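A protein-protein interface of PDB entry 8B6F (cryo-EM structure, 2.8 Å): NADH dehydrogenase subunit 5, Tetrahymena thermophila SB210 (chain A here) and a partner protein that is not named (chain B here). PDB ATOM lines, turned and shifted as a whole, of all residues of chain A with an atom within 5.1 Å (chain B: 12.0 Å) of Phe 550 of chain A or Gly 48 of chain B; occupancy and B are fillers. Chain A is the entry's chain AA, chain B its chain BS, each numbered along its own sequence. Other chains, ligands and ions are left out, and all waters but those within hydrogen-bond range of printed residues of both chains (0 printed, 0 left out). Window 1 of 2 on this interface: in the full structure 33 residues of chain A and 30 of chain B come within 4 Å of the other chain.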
ATOM      1  N   LEU A 548      10.954 -11.849   9.139  1.00  0.00           N
ATOM      2  CA  LEU A 548      10.129 -10.646   9.237  1.00  0.00           C
ATOM      3  C   LEU A 548       9.088 -10.854  10.326  1.00  0.00           C
ATOM      4  O   LEU A 548       7.892 -10.986  10.046  1.00  0.00           O
ATOM      5  CB  LEU A 548       9.462 -10.326   7.900  1.00  0.00           C
ATOM      6  CG  LEU A 548      10.382 -10.217   6.684  1.00  0.00           C
ATOM      7  CD1 LEU A 548       9.566 -10.199   5.411  1.00  0.00           C
ATOM      8  CD2 LEU A 548      11.237  -8.972   6.778  1.00  0.00           C
ATOM      9  N   PRO A 549       9.514 -10.894  11.591  1.00  0.00           N
ATOM     10  CA  PRO A 549       8.544 -11.167  12.666  1.00  0.00           C
ATOM     11  C   PRO A 549       7.408 -10.163  12.722  1.00  0.00           C
ATOM     12  O   PRO A 549       6.240 -10.556  12.821  1.00  0.00           O
ATOM     13  CB  PRO A 549       9.412 -11.125  13.934  1.00  0.00           C
ATOM     14  CG  PRO A 549      10.805 -11.314  13.462  1.00  0.00           C
ATOM     15  CD  PRO A 549      10.872 -10.688  12.115  1.00  0.00           C
ATOM     16  N   PHE A 550       7.718  -8.867  12.659  1.00  0.00           N
ATOM     17  CA  PHE A 550       6.668  -7.859  12.732  1.00  0.00           C
ATOM     18  C   PHE A 550       5.704  -7.981  11.562  1.00  0.00           C
ATOM     19  O   PHE A 550       4.486  -7.870  11.737  1.00  0.00           O
ATOM     20  CB  PHE A 550       7.283  -6.461  12.768  1.00  0.00           C
ATOM     21  CG  PHE A 550       6.270  -5.357  12.677  1.00  0.00           C
ATOM     22  CD1 PHE A 550       5.662  -4.867  13.818  1.00  0.00           C
ATOM     23  CD2 PHE A 550       5.927  -4.811  11.452  1.00  0.00           C
ATOM     24  CE1 PHE A 550       4.729  -3.855  13.739  1.00  0.00           C
ATOM     25  CE2 PHE A 550       4.996  -3.799  11.369  1.00  0.00           C
ATOM     26  CZ  PHE A 550       4.396  -3.320  12.513  1.00  0.00           C
ATOM     27  N   GLU A 551       6.229  -8.204  10.356  1.00  0.00           N
ATOM     28  CA  GLU A 551       5.362  -8.296   9.187  1.00  0.00           C
ATOM     29  C   GLU A 551       4.381  -9.450   9.325  1.00  0.00           C
ATOM     30  O   GLU A 551       3.214  -9.333   8.935  1.00  0.00           O
ATOM     31  CB  GLU A 551       6.200  -8.455   7.920  1.00  0.00           C
ATOM     32  CG  GLU A 551       6.818  -7.162   7.409  1.00  0.00           C
ATOM     33  CD  GLU A 551       7.835  -6.570   8.365  1.00  0.00           C
ATOM     34  OE1 GLU A 551       8.165  -7.227   9.373  1.00  0.00           O
ATOM     35  OE2 GLU A 551       8.308  -5.445   8.104  1.00  0.00           O
ATOM     36  N   CYS A 552       4.838 -10.582   9.866  1.00  0.00           N
ATOM     37  CA  CYS A 552       3.958 -11.736  10.003  1.00  0.00           C
ATOM     38  C   CYS A 552       2.744 -11.396  10.857  1.00  0.00           C
ATOM     39  O   CYS A 552       1.600 -11.616  10.447  1.00  0.00           O
ATOM     40  CB  CYS A 552       4.729 -12.909  10.608  1.00  0.00           C
ATOM     41  SG  CYS A 552       3.719 -14.366  10.926  1.00  0.00           S
ATOM     42  N   LEU A 553       2.976 -10.853  12.053  1.00  0.00           N
ATOM     43  CA  LEU A 553       1.868 -10.586  12.962  1.00  0.00           C
ATOM     44  C   LEU A 553       1.008  -9.434  12.462  1.00  0.00           C
ATOM     45  O   LEU A 553      -0.224  -9.488  12.547  1.00  0.00           O
ATOM     46  CB  LEU A 553       2.406 -10.300  14.363  1.00  0.00           C
ATOM     47  CG  LEU A 553       3.227 -11.453  14.947  1.00  0.00           C
ATOM     48  CD1 LEU A 553       4.001 -11.023  16.168  1.00  0.00           C
ATOM     49  CD2 LEU A 553       2.318 -12.616  15.289  1.00  0.00           C
ATOM     50  N   ALA A 554       1.637  -8.382  11.937  1.00  0.00           N
ATOM     51  CA  ALA A 554       0.876  -7.270  11.382  1.00  0.00           C
ATOM     52  C   ALA A 554       0.006  -7.731  10.222  1.00  0.00           C
ATOM     53  O   ALA A 554      -1.161  -7.338  10.114  1.00  0.00           O
ATOM     54  CB  ALA A 554       1.819  -6.154  10.933  1.00  0.00           C
ATOM     55  N   SER A 555       0.560  -8.567   9.343  1.00  0.00           N
ATOM     56  CA  SER A 555      -0.222  -9.102   8.235  1.00  0.00           C
ATOM     57  C   SER A 555      -1.356  -9.982   8.734  1.00  0.00           C
ATOM     58  O   SER A 555      -2.465  -9.943   8.190  1.00  0.00           O
ATOM     59  CB  SER A 555       0.681  -9.895   7.290  1.00  0.00           C
ATOM     60  OG  SER A 555       1.748  -9.101   6.806  1.00  0.00           O
ATOM     61  N   SER A 645       9.285   2.018   9.545  1.00  0.00           N
ATOM     62  CA  SER A 645       8.207   1.300   8.872  1.00  0.00           C
ATOM     63  C   SER A 645       7.333   0.554   9.870  1.00  0.00           C
ATOM     64  O   SER A 645       6.102   0.589   9.775  1.00  0.00           O
ATOM     65  CB  SER A 645       8.791   0.317   7.862  1.00  0.00           C
ATOM     66  OG  SER A 645       7.774  -0.473   7.274  1.00  0.00           O
ATOM     67  N   ASN A 646       7.950  -0.131  10.833  1.00  0.00           N
ATOM     68  CA  ASN A 646       7.169  -0.851  11.831  1.00  0.00           C
ATOM     69  C   ASN A 646       6.297   0.103  12.634  1.00  0.00           C
ATOM     70  O   ASN A 646       5.114  -0.167  12.865  1.00  0.00           O
ATOM     71  CB  ASN A 646       8.098  -1.634  12.757  1.00  0.00           C
ATOM     72  CG  ASN A 646       8.950  -2.636  12.010  1.00  0.00           C
ATOM     73  OD1 ASN A 646       8.617  -3.046  10.899  1.00  0.00           O
ATOM     74  ND2 ASN A 646      10.060  -3.039  12.617  1.00  0.00           N
ATOM     75  N   ILE A 649       3.334   1.361  10.522  1.00  0.00           N
ATOM     76  CA  ILE A 649       2.281   0.360  10.380  1.00  0.00           C
ATOM     77  C   ILE A 649       1.504   0.214  11.682  1.00  0.00           C
ATOM     78  O   ILE A 649       0.270   0.123  11.678  1.00  0.00           O
ATOM     79  CB  ILE A 649       2.878  -0.982   9.914  1.00  0.00           C
ATOM     80  CG1 ILE A 649       3.415  -0.839   8.488  1.00  0.00           C
ATOM     81  CG2 ILE A 649       1.832  -2.094   9.982  1.00  0.00           C
ATOM     82  CD1 ILE A 649       4.181  -2.042   7.988  1.00  0.00           C
ATOM     83  N   THR A 650       2.207   0.185  12.816  1.00  0.00           N
ATOM     84  CA  THR A 650       1.531   0.041  14.102  1.00  0.00           C
ATOM     85  C   THR A 650       0.581   1.203  14.355  1.00  0.00           C
ATOM     86  O   THR A 650      -0.573   1.003  14.751  1.00  0.00           O
ATOM     87  CB  THR A 650       2.563  -0.060  15.227  1.00  0.00           C
ATOM     88  OG1 THR A 650       3.408  -1.196  15.007  1.00  0.00           O
ATOM     89  CG2 THR A 650       1.877  -0.207  16.580  1.00  0.00           C
ATOM     90  N   LEU B  37      18.766 -19.493  11.241  1.00  0.00           N
ATOM     91  CA  LEU B  37      18.946 -18.199  11.883  1.00  0.00           C
ATOM     92  C   LEU B  37      18.906 -18.418  13.390  1.00  0.00           C
ATOM     93  O   LEU B  37      17.937 -18.979  13.912  1.00  0.00           O
ATOM     94  CB  LEU B  37      17.862 -17.215  11.442  1.00  0.00           C
ATOM     95  CG  LEU B  37      17.897 -15.817  12.064  1.00  0.00           C
ATOM     96  CD1 LEU B  37      19.130 -15.049  11.634  1.00  0.00           C
ATOM     97  CD2 LEU B  37      16.641 -15.051  11.692  1.00  0.00           C
ATOM     98  N   TRP B  39      18.583 -16.414  15.918  1.00  0.00           N
ATOM     99  CA  TRP B  39      17.907 -15.426  16.746  1.00  0.00           C
ATOM    100  C   TRP B  39      16.725 -14.877  15.961  1.00  0.00           C
ATOM    101  O   TRP B  39      16.441 -15.312  14.841  1.00  0.00           O
ATOM    102  CB  TRP B  39      18.870 -14.309  17.153  1.00  0.00           C
ATOM    103  CG  TRP B  39      19.408 -13.571  15.973  1.00  0.00           C
ATOM    104  CD1 TRP B  39      18.953 -12.390  15.470  1.00  0.00           C
ATOM    105  CD2 TRP B  39      20.493 -13.975  15.130  1.00  0.00           C
ATOM    106  NE1 TRP B  39      19.691 -12.030  14.370  1.00  0.00           N
ATOM    107  CE2 TRP B  39      20.642 -12.988  14.141  1.00  0.00           C
ATOM    108  CE3 TRP B  39      21.354 -15.076  15.120  1.00  0.00           C
ATOM    109  CZ2 TRP B  39      21.618 -13.065  13.151  1.00  0.00           C
ATOM    110  CZ3 TRP B  39      22.321 -15.152  14.138  1.00  0.00           C
ATOM    111  CH2 TRP B  39      22.446 -14.152  13.166  1.00  0.00           C
ATOM    112  N   ILE B  40      16.037 -13.910  16.558  1.00  0.00           N
ATOM    113  CA  ILE B  40      14.937 -13.211  15.906  1.00  0.00           C
ATOM    114  C   ILE B  40      15.077 -11.731  16.228  1.00  0.00           C
ATOM    115  O   ILE B  40      15.437 -11.360  17.349  1.00  0.00           O
ATOM    116  CB  ILE B  40      13.563 -13.750  16.358  1.00  0.00           C
ATOM    117  CG1 ILE B  40      13.526 -15.274  16.200  1.00  0.00           C
ATOM    118  CG2 ILE B  40      12.453 -13.083  15.559  1.00  0.00           C
ATOM    119  CD1 ILE B  40      12.171 -15.917  16.468  1.00  0.00           C
ATOM    120  N   SER B  41      14.808 -10.888  15.235  1.00  0.00           N
ATOM    121  CA  SER B  41      14.906  -9.446  15.415  1.00  0.00           C
ATOM    122  C   SER B  41      14.162  -9.007  16.667  1.00  0.00           C
ATOM    123  O   SER B  41      12.947  -9.189  16.776  1.00  0.00           O
ATOM    124  CB  SER B  41      14.351  -8.733  14.182  1.00  0.00           C
ATOM    125  OG  SER B  41      14.315  -7.333  14.386  1.00  0.00           O
ATOM    126  N   ASN B  42      14.902  -8.430  17.615  1.00  0.00           N
ATOM    127  CA  ASN B  42      14.327  -8.113  18.918  1.00  0.00           C
ATOM    128  C   ASN B  42      13.260  -7.032  18.805  1.00  0.00           C
ATOM    129  O   ASN B  42      12.139  -7.199  19.299  1.00  0.00           O
ATOM    130  CB  ASN B  42      15.433  -7.678  19.879  1.00  0.00           C
ATOM    131  CG  ASN B  42      14.932  -7.483  21.294  1.00  0.00           C
ATOM    132  OD1 ASN B  42      14.723  -8.446  22.028  1.00  0.00           O
ATOM    133  ND2 ASN B  42      14.746  -6.229  21.688  1.00  0.00           N
ATOM    134  N   VAL B  43      13.587  -5.914  18.158  1.00  0.00           N
ATOM    135  CA  VAL B  43      12.640  -4.805  18.079  1.00  0.00           C
ATOM    136  C   VAL B  43      11.436  -5.187  17.226  1.00  0.00           C
ATOM    137  O   VAL B  43      10.290  -4.880  17.574  1.00  0.00           O
ATOM    138  CB  VAL B  43      13.337  -3.541  17.548  1.00  0.00           C
ATOM    139  CG1 VAL B  43      12.378  -2.367  17.555  1.00  0.00           C
ATOM    140  CG2 VAL B  43      14.572  -3.220  18.377  1.00  0.00           C
ATOM    141  N   ASP B  44      11.671  -5.848  16.091  1.00  0.00           N
ATOM    142  CA  ASP B  44      10.563  -6.277  15.244  1.00  0.00           C
ATOM    143  C   ASP B  44       9.640  -7.234  15.984  1.00  0.00           C
ATOM    144  O   ASP B  44       8.414  -7.105  15.912  1.00  0.00           O
ATOM    145  CB  ASP B  44      11.092  -6.935  13.971  1.00  0.00           C
ATOM    146  CG  ASP B  44      11.885  -5.981  13.109  1.00  0.00           C
ATOM    147  OD1 ASP B  44      12.002  -4.796  13.485  1.00  0.00           O
ATOM    148  OD2 ASP B  44      12.397  -6.419  12.058  1.00  0.00           O
ATOM    149  N   LEU B  45      10.210  -8.200  16.705  1.00  0.00           N
ATOM    150  CA  LEU B  45       9.381  -9.143  17.443  1.00  0.00           C
ATOM    151  C   LEU B  45       8.588  -8.439  18.536  1.00  0.00           C
ATOM    152  O   LEU B  45       7.408  -8.742  18.745  1.00  0.00           O
ATOM    153  CB  LEU B  45      10.248 -10.248  18.045  1.00  0.00           C
ATOM    154  CG  LEU B  45       9.490 -11.380  18.743  1.00  0.00           C
ATOM    155  CD1 LEU B  45       8.623 -12.143  17.756  1.00  0.00           C
ATOM    156  CD2 LEU B  45      10.451 -12.318  19.441  1.00  0.00           C
ATOM    157  N   ARG B  46       9.210  -7.494  19.241  1.00  0.00           N
ATOM    158  CA  ARG B  46       8.485  -6.775  20.283  1.00  0.00           C
ATOM    159  C   ARG B  46       7.301  -6.018  19.696  1.00  0.00           C
ATOM    160  O   ARG B  46       6.182  -6.094  20.216  1.00  0.00           O
ATOM    161  CB  ARG B  46       9.428  -5.815  21.009  1.00  0.00           C
ATOM    162  CG  ARG B  46      10.448  -6.496  21.906  1.00  0.00           C
ATOM    163  CD  ARG B  46       9.776  -7.232  23.052  1.00  0.00           C
ATOM    164  NE  ARG B  46      10.727  -7.604  24.093  1.00  0.00           N
ATOM    165  CZ  ARG B  46      10.413  -8.292  25.182  1.00  0.00           C
ATOM    166  NH1 ARG B  46       9.181  -8.718  25.399  1.00  0.00           N
ATOM    167  NH2 ARG B  46      11.360  -8.556  26.077  1.00  0.00           N
ATOM    168  N   LEU B  47       7.528  -5.272  18.611  1.00  0.00           N
ATOM    169  CA  LEU B  47       6.437  -4.516  18.006  1.00  0.00           C
ATOM    170  C   LEU B  47       5.366  -5.446  17.457  1.00  0.00           C
ATOM    171  O   LEU B  47       4.167  -5.186  17.609  1.00  0.00           O
ATOM    172  CB  LEU B  47       6.969  -3.604  16.900  1.00  0.00           C
ATOM    173  CG  LEU B  47       7.880  -2.458  17.343  1.00  0.00           C
ATOM    174  CD1 LEU B  47       8.381  -1.689  16.134  1.00  0.00           C
ATOM    175  CD2 LEU B  47       7.158  -1.526  18.303  1.00  0.00           C
ATOM    176  N   GLY B  48       5.781  -6.538  16.817  1.00  0.00           N
ATOM    177  CA  GLY B  48       4.813  -7.483  16.291  1.00  0.00           C
ATOM    178  C   GLY B  48       3.970  -8.115  17.380  1.00  0.00           C
ATOM    179  O   GLY B  48       2.756  -8.271  17.229  1.00  0.00           O
ATOM    180  N   ARG B  49       4.600  -8.494  18.491  1.00  0.00           N
ATOM    181  CA  ARG B  49       3.848  -9.063  19.602  1.00  0.00           C
ATOM    182  C   ARG B  49       2.901  -8.038  20.210  1.00  0.00           C
ATOM    183  O   ARG B  49       1.787  -8.383  20.621  1.00  0.00           O
ATOM    184  CB  ARG B  49       4.808  -9.606  20.661  1.00  0.00           C
ATOM    185  CG  ARG B  49       5.626 -10.810  20.204  1.00  0.00           C
ATOM    186  CD  ARG B  49       4.753 -12.028  19.932  1.00  0.00           C
ATOM    187  NE  ARG B  49       4.007 -12.439  21.114  1.00  0.00           N
ATOM    188  CZ  ARG B  49       3.089 -13.394  21.128  1.00  0.00           C
ATOM    189  NH1 ARG B  49       2.762 -14.056  20.030  1.00  0.00           N
ATOM    190  NH2 ARG B  49       2.482 -13.694  22.273  1.00  0.00           N
ATOM    191  N   ALA B  50       3.324  -6.774  20.283  1.00  0.00           N
ATOM    192  CA  ALA B  50       2.439  -5.733  20.794  1.00  0.00           C
ATOM    193  C   ALA B  50       1.194  -5.594  19.927  1.00  0.00           C
ATOM    194  O   ALA B  50       0.070  -5.541  20.439  1.00  0.00           O
ATOM    195  CB  ALA B  50       3.192  -4.405  20.873  1.00  0.00           C
ATOM    196  N   ILE B  51       1.374  -5.518  18.608  1.00  0.00           N
ATOM    197  CA  ILE B  51       0.225  -5.349  17.722  1.00  0.00           C
ATOM    198  C   ILE B  51      -0.634  -6.606  17.722  1.00  0.00           C
ATOM    199  O   ILE B  51      -1.866  -6.534  17.654  1.00  0.00           O
ATOM    200  CB  ILE B  51       0.685  -4.965  16.303  1.00  0.00           C
ATOM    201  CG1 ILE B  51      -0.531  -4.668  15.424  1.00  0.00           C
ATOM    202  CG2 ILE B  51       1.532  -6.063  15.692  1.00  0.00           C
ATOM    203  CD1 ILE B  51      -0.188  -4.069  14.082  1.00  0.00           C
ATOM    204  N   PHE B  52       0.000  -7.778  17.799  1.00  0.00           N
ATOM    205  CA  PHE B  52      -0.753  -9.026  17.881  1.00  0.00           C
ATOM    206  C   PHE B  52      -1.587  -9.071  19.153  1.00  0.00           C
ATOM    207  O   PHE B  52      -2.744  -9.505  19.133  1.00  0.00           O
ATOM    208  CB  PHE B  52       0.204 -10.218  17.818  1.00  0.00           C
ATOM    209  CG  PHE B  52      -0.476 -11.552  17.952  1.00  0.00           C
ATOM    210  CD1 PHE B  52      -1.078 -12.151  16.859  1.00  0.00           C
ATOM    211  CD2 PHE B  52      -0.492 -12.217  19.167  1.00  0.00           C
ATOM    212  CE1 PHE B  52      -1.697 -13.381  16.979  1.00  0.00           C
ATOM    213  CE2 PHE B  52      -1.109 -13.446  19.293  1.00  0.00           C
ATOM    214  CZ  PHE B  52      -1.710 -14.028  18.198  1.00  0.00           C
ATOM    215  N   THR B  53      -1.019  -8.616  20.271  1.00  0.00           N
ATOM    216  CA  THR B  53      -1.779  -8.556  21.515  1.00  0.00           C
ATOM    217  C   THR B  53      -2.947  -7.589  21.397  1.00  0.00           C
ATOM    218  O   THR B  53      -4.048  -7.873  21.879  1.00  0.00           O
ATOM    219  CB  THR B  53      -0.863  -8.149  22.667  1.00  0.00           C
ATOM    220  OG1 THR B  53       0.206  -9.093  22.789  1.00  0.00           O
ATOM    221  CG2 THR B  53      -1.638  -8.087  23.976  1.00  0.00           C
ATOM    222  N   PHE B  54      -2.730  -6.442  20.753  1.00  0.00           N
ATOM    223  CA  PHE B  54      -3.822  -5.499  20.539  1.00  0.00           C
ATOM    224  C   PHE B  54      -4.944  -6.145  19.736  1.00  0.00           C
ATOM    225  O   PHE B  54      -6.125  -5.999  20.068  1.00  0.00           O
ATOM    226  CB  PHE B  54      -3.293  -4.248  19.837  1.00  0.00           C
ATOM    227  CG  PHE B  54      -4.352  -3.236  19.526  1.00  0.00           C
ATOM    228  CD1 PHE B  54      -4.772  -2.340  20.495  1.00  0.00           C
ATOM    229  CD2 PHE B  54      -4.916  -3.166  18.265  1.00  0.00           C
ATOM    230  CE1 PHE B  54      -5.743  -1.402  20.215  1.00  0.00           C
ATOM    231  CE2 PHE B  54      -5.887  -2.230  17.976  1.00  0.00           C
ATOM    232  CZ  PHE B  54      -6.301  -1.345  18.953  1.00  0.00           C
ATOM    233  N   GLY B  55      -4.591  -6.860  18.668  1.00  0.00           N
ATOM    234  CA  GLY B  55      -5.607  -7.527  17.868  1.00  0.00           C
ATOM    235  C   GLY B  55      -6.343  -8.608  18.637  1.00  0.00           C
ATOM    236  O   GLY B  55      -7.561  -8.750  18.513  1.00  0.00           O
ATOM    237  N   VAL B  56      -5.616  -9.385  19.441  1.00  0.00           N
ATOM    238  CA  VAL B  56      -6.247 -10.431  20.242  1.00  0.00           C
ATOM    239  C   VAL B  56      -7.211  -9.822  21.252  1.00  0.00           C
ATOM    240  O   VAL B  56      -8.320 -10.329  21.459  1.00  0.00           O
ATOM    241  CB  VAL B  56      -5.176 -11.299  20.930  1.00  0.00           C
ATOM    242  CG1 VAL B  56      -5.806 -12.228  21.963  1.00  0.00           C
ATOM    243  CG2 VAL B  56      -4.410 -12.107  19.900  1.00  0.00           C
ATOM    244  N   VAL B  57      -6.807  -8.729  21.900  1.00  0.00           N
ATOM    245  CA  VAL B  57      -7.695  -8.062  22.848  1.00  0.00           C
ATOM    246  C   VAL B  57      -8.946  -7.566  22.138  1.00  0.00           C
ATOM    247  O   VAL B  57     -10.060  -7.675  22.663  1.00  0.00           O
ATOM    248  CB  VAL B  57      -6.953  -6.916  23.563  1.00  0.00           C
ATOM    249  CG1 VAL B  57      -7.911  -6.100  24.420  1.00  0.00           C
ATOM    250  CG2 VAL B  57      -5.833  -7.466  24.426  1.00  0.00           C
ATOM    251  N   ILE B  59     -10.321  -8.842  19.399  1.00  0.00           N
ATOM    252  CA  ILE B  59     -11.147  -9.998  19.061  1.00  0.00           C
ATOM    253  C   ILE B  59     -11.899 -10.488  20.290  1.00  0.00           C
ATOM    254  O   ILE B  59     -13.086 -10.824  20.218  1.00  0.00           O
ATOM    255  CB  ILE B  59     -10.275 -11.111  18.450  1.00  0.00           C
ATOM    256  CG1 ILE B  59      -9.740 -10.671  17.087  1.00  0.00           C
ATOM    257  CG2 ILE B  59     -11.067 -12.408  18.319  1.00  0.00           C
ATOM    258  CD1 ILE B  59      -8.693 -11.600  16.510  1.00  0.00           C
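The side-chain hydroxyl (OG) of Ser 41 of chain B sits close to the side-chain carboxylate (OD2) of Asp 44 of chain B, 3.2 Å away. The backbone carbonyl oxygen (O) of Arg 49 of chain B sits at hydrogen-bond distance from the side-chain hydroxyl (OG1) of Thr 53 of chain B (2.8 Å). The side-chain hydroxyl (OG1) of Thr 650 of chain A lies within hydrogen-bond range of the backbone carbonyl oxygen (O) of Asn 646 of chain A.
The side-chain amide nitrogen (ND2) of Asn 646 of chain A sits at hydrogen-bond distance from the side-chain carboxylate (OD1) of Asp 44 of chain B, at 2.8 Å.
Of the 21 printed residues of chain B, 6 touch a printed residue of chain A. Printed residues of chain B that touch a printed residue of chain A: Ile 40, Asp 44, Leu 47, Gly 48, Arg 49 and Phe 52. Hydrophobic or aromatic side chains of chain B that line the printed part of chain A: Ile 40, Leu 47 and Phe 52. Along chain B the printed residues that touch a printed residue of chain A span positions 40 to 52. Of the 12 printed residues of chain A, 4 touch a printed residue of chain B. Printed residues of chain A that touch a printed residue of chain B: Pro 549, Phe 550, Leu 553 and Asn 646. Hydrophobic or aromatic side chains of chain A within 4 Å of the printed part of chain B: Pro 549, Phe 550 and Leu 553. Among the printed residues, 9 pairs touch across the chains. Among the printed residues, no Asp or Glu carboxylate lies within 4 Å of a Lys or Arg side-chain nitrogen of the other chain.
Ile 40 of chain B touches Pro 549 of chain A. Phe 550 of chain A touches Asp 44 of chain B (CB to O, 3.4 Å). Phe 550 of chain A touches Leu 47 of chain B (CD1 to CB, 3.6 Å). N of Gly 48 of chain B touches CD1 of Phe 550 of chain A, at 3.4 Å. Gly 48 of chain B touches Leu 553 of chain A. CD1 of Leu 553 of chain A touches N of Arg 49 of chain B, at 3.5 Å. Phe 52 of chain B touches Leu 553 of chain A (CD1 to CD2, 3.8 Å). Leu 47 of chain B touches Asn 646 of chain A (CD1 to CB, 3.4 Å).
Leu 548 of chain A touches none of the printed residues of chain B. Pro 549 of chain A touches just one residue of chain B: Ile 40. Of chain B, only Asp 44, Leu 47 and Gly 48 come within 4 Å of Phe 550 of chain A. No residue of chain B comes within 4 Å of Cys 552 of chain A. Ser 645 of chain A touches none of the printed residues of chain B. Of chain B, only Asp 44 (2.8 Å) and Leu 47 (3.4 Å) come within 4 Å of Asn 646 of chain A. Printed residues of chain A within 4 Å of Ile 40 of chain B: Pro 549 (3.2 Å). Printed residues of chain A within 4 Å of Asp 44 of chain B: Phe 550 (3.4 Å) and Asn 646 (2.8 Å). Printed residues of chain A within 4 Å of Leu 47 of chain B: Phe 550 and Asn 646. Gly 48 of chain B touches two residues of chain A. Of the printed residues of chain A, Arg 49 of chain B touches Leu 553. Of the printed residues of chain A, Phe 52 of chain B touches Leu 553. The nearest printed residue of chain A that does not touch Ile 40 of chain B is Leu 548 of chain A (6.6 Å).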
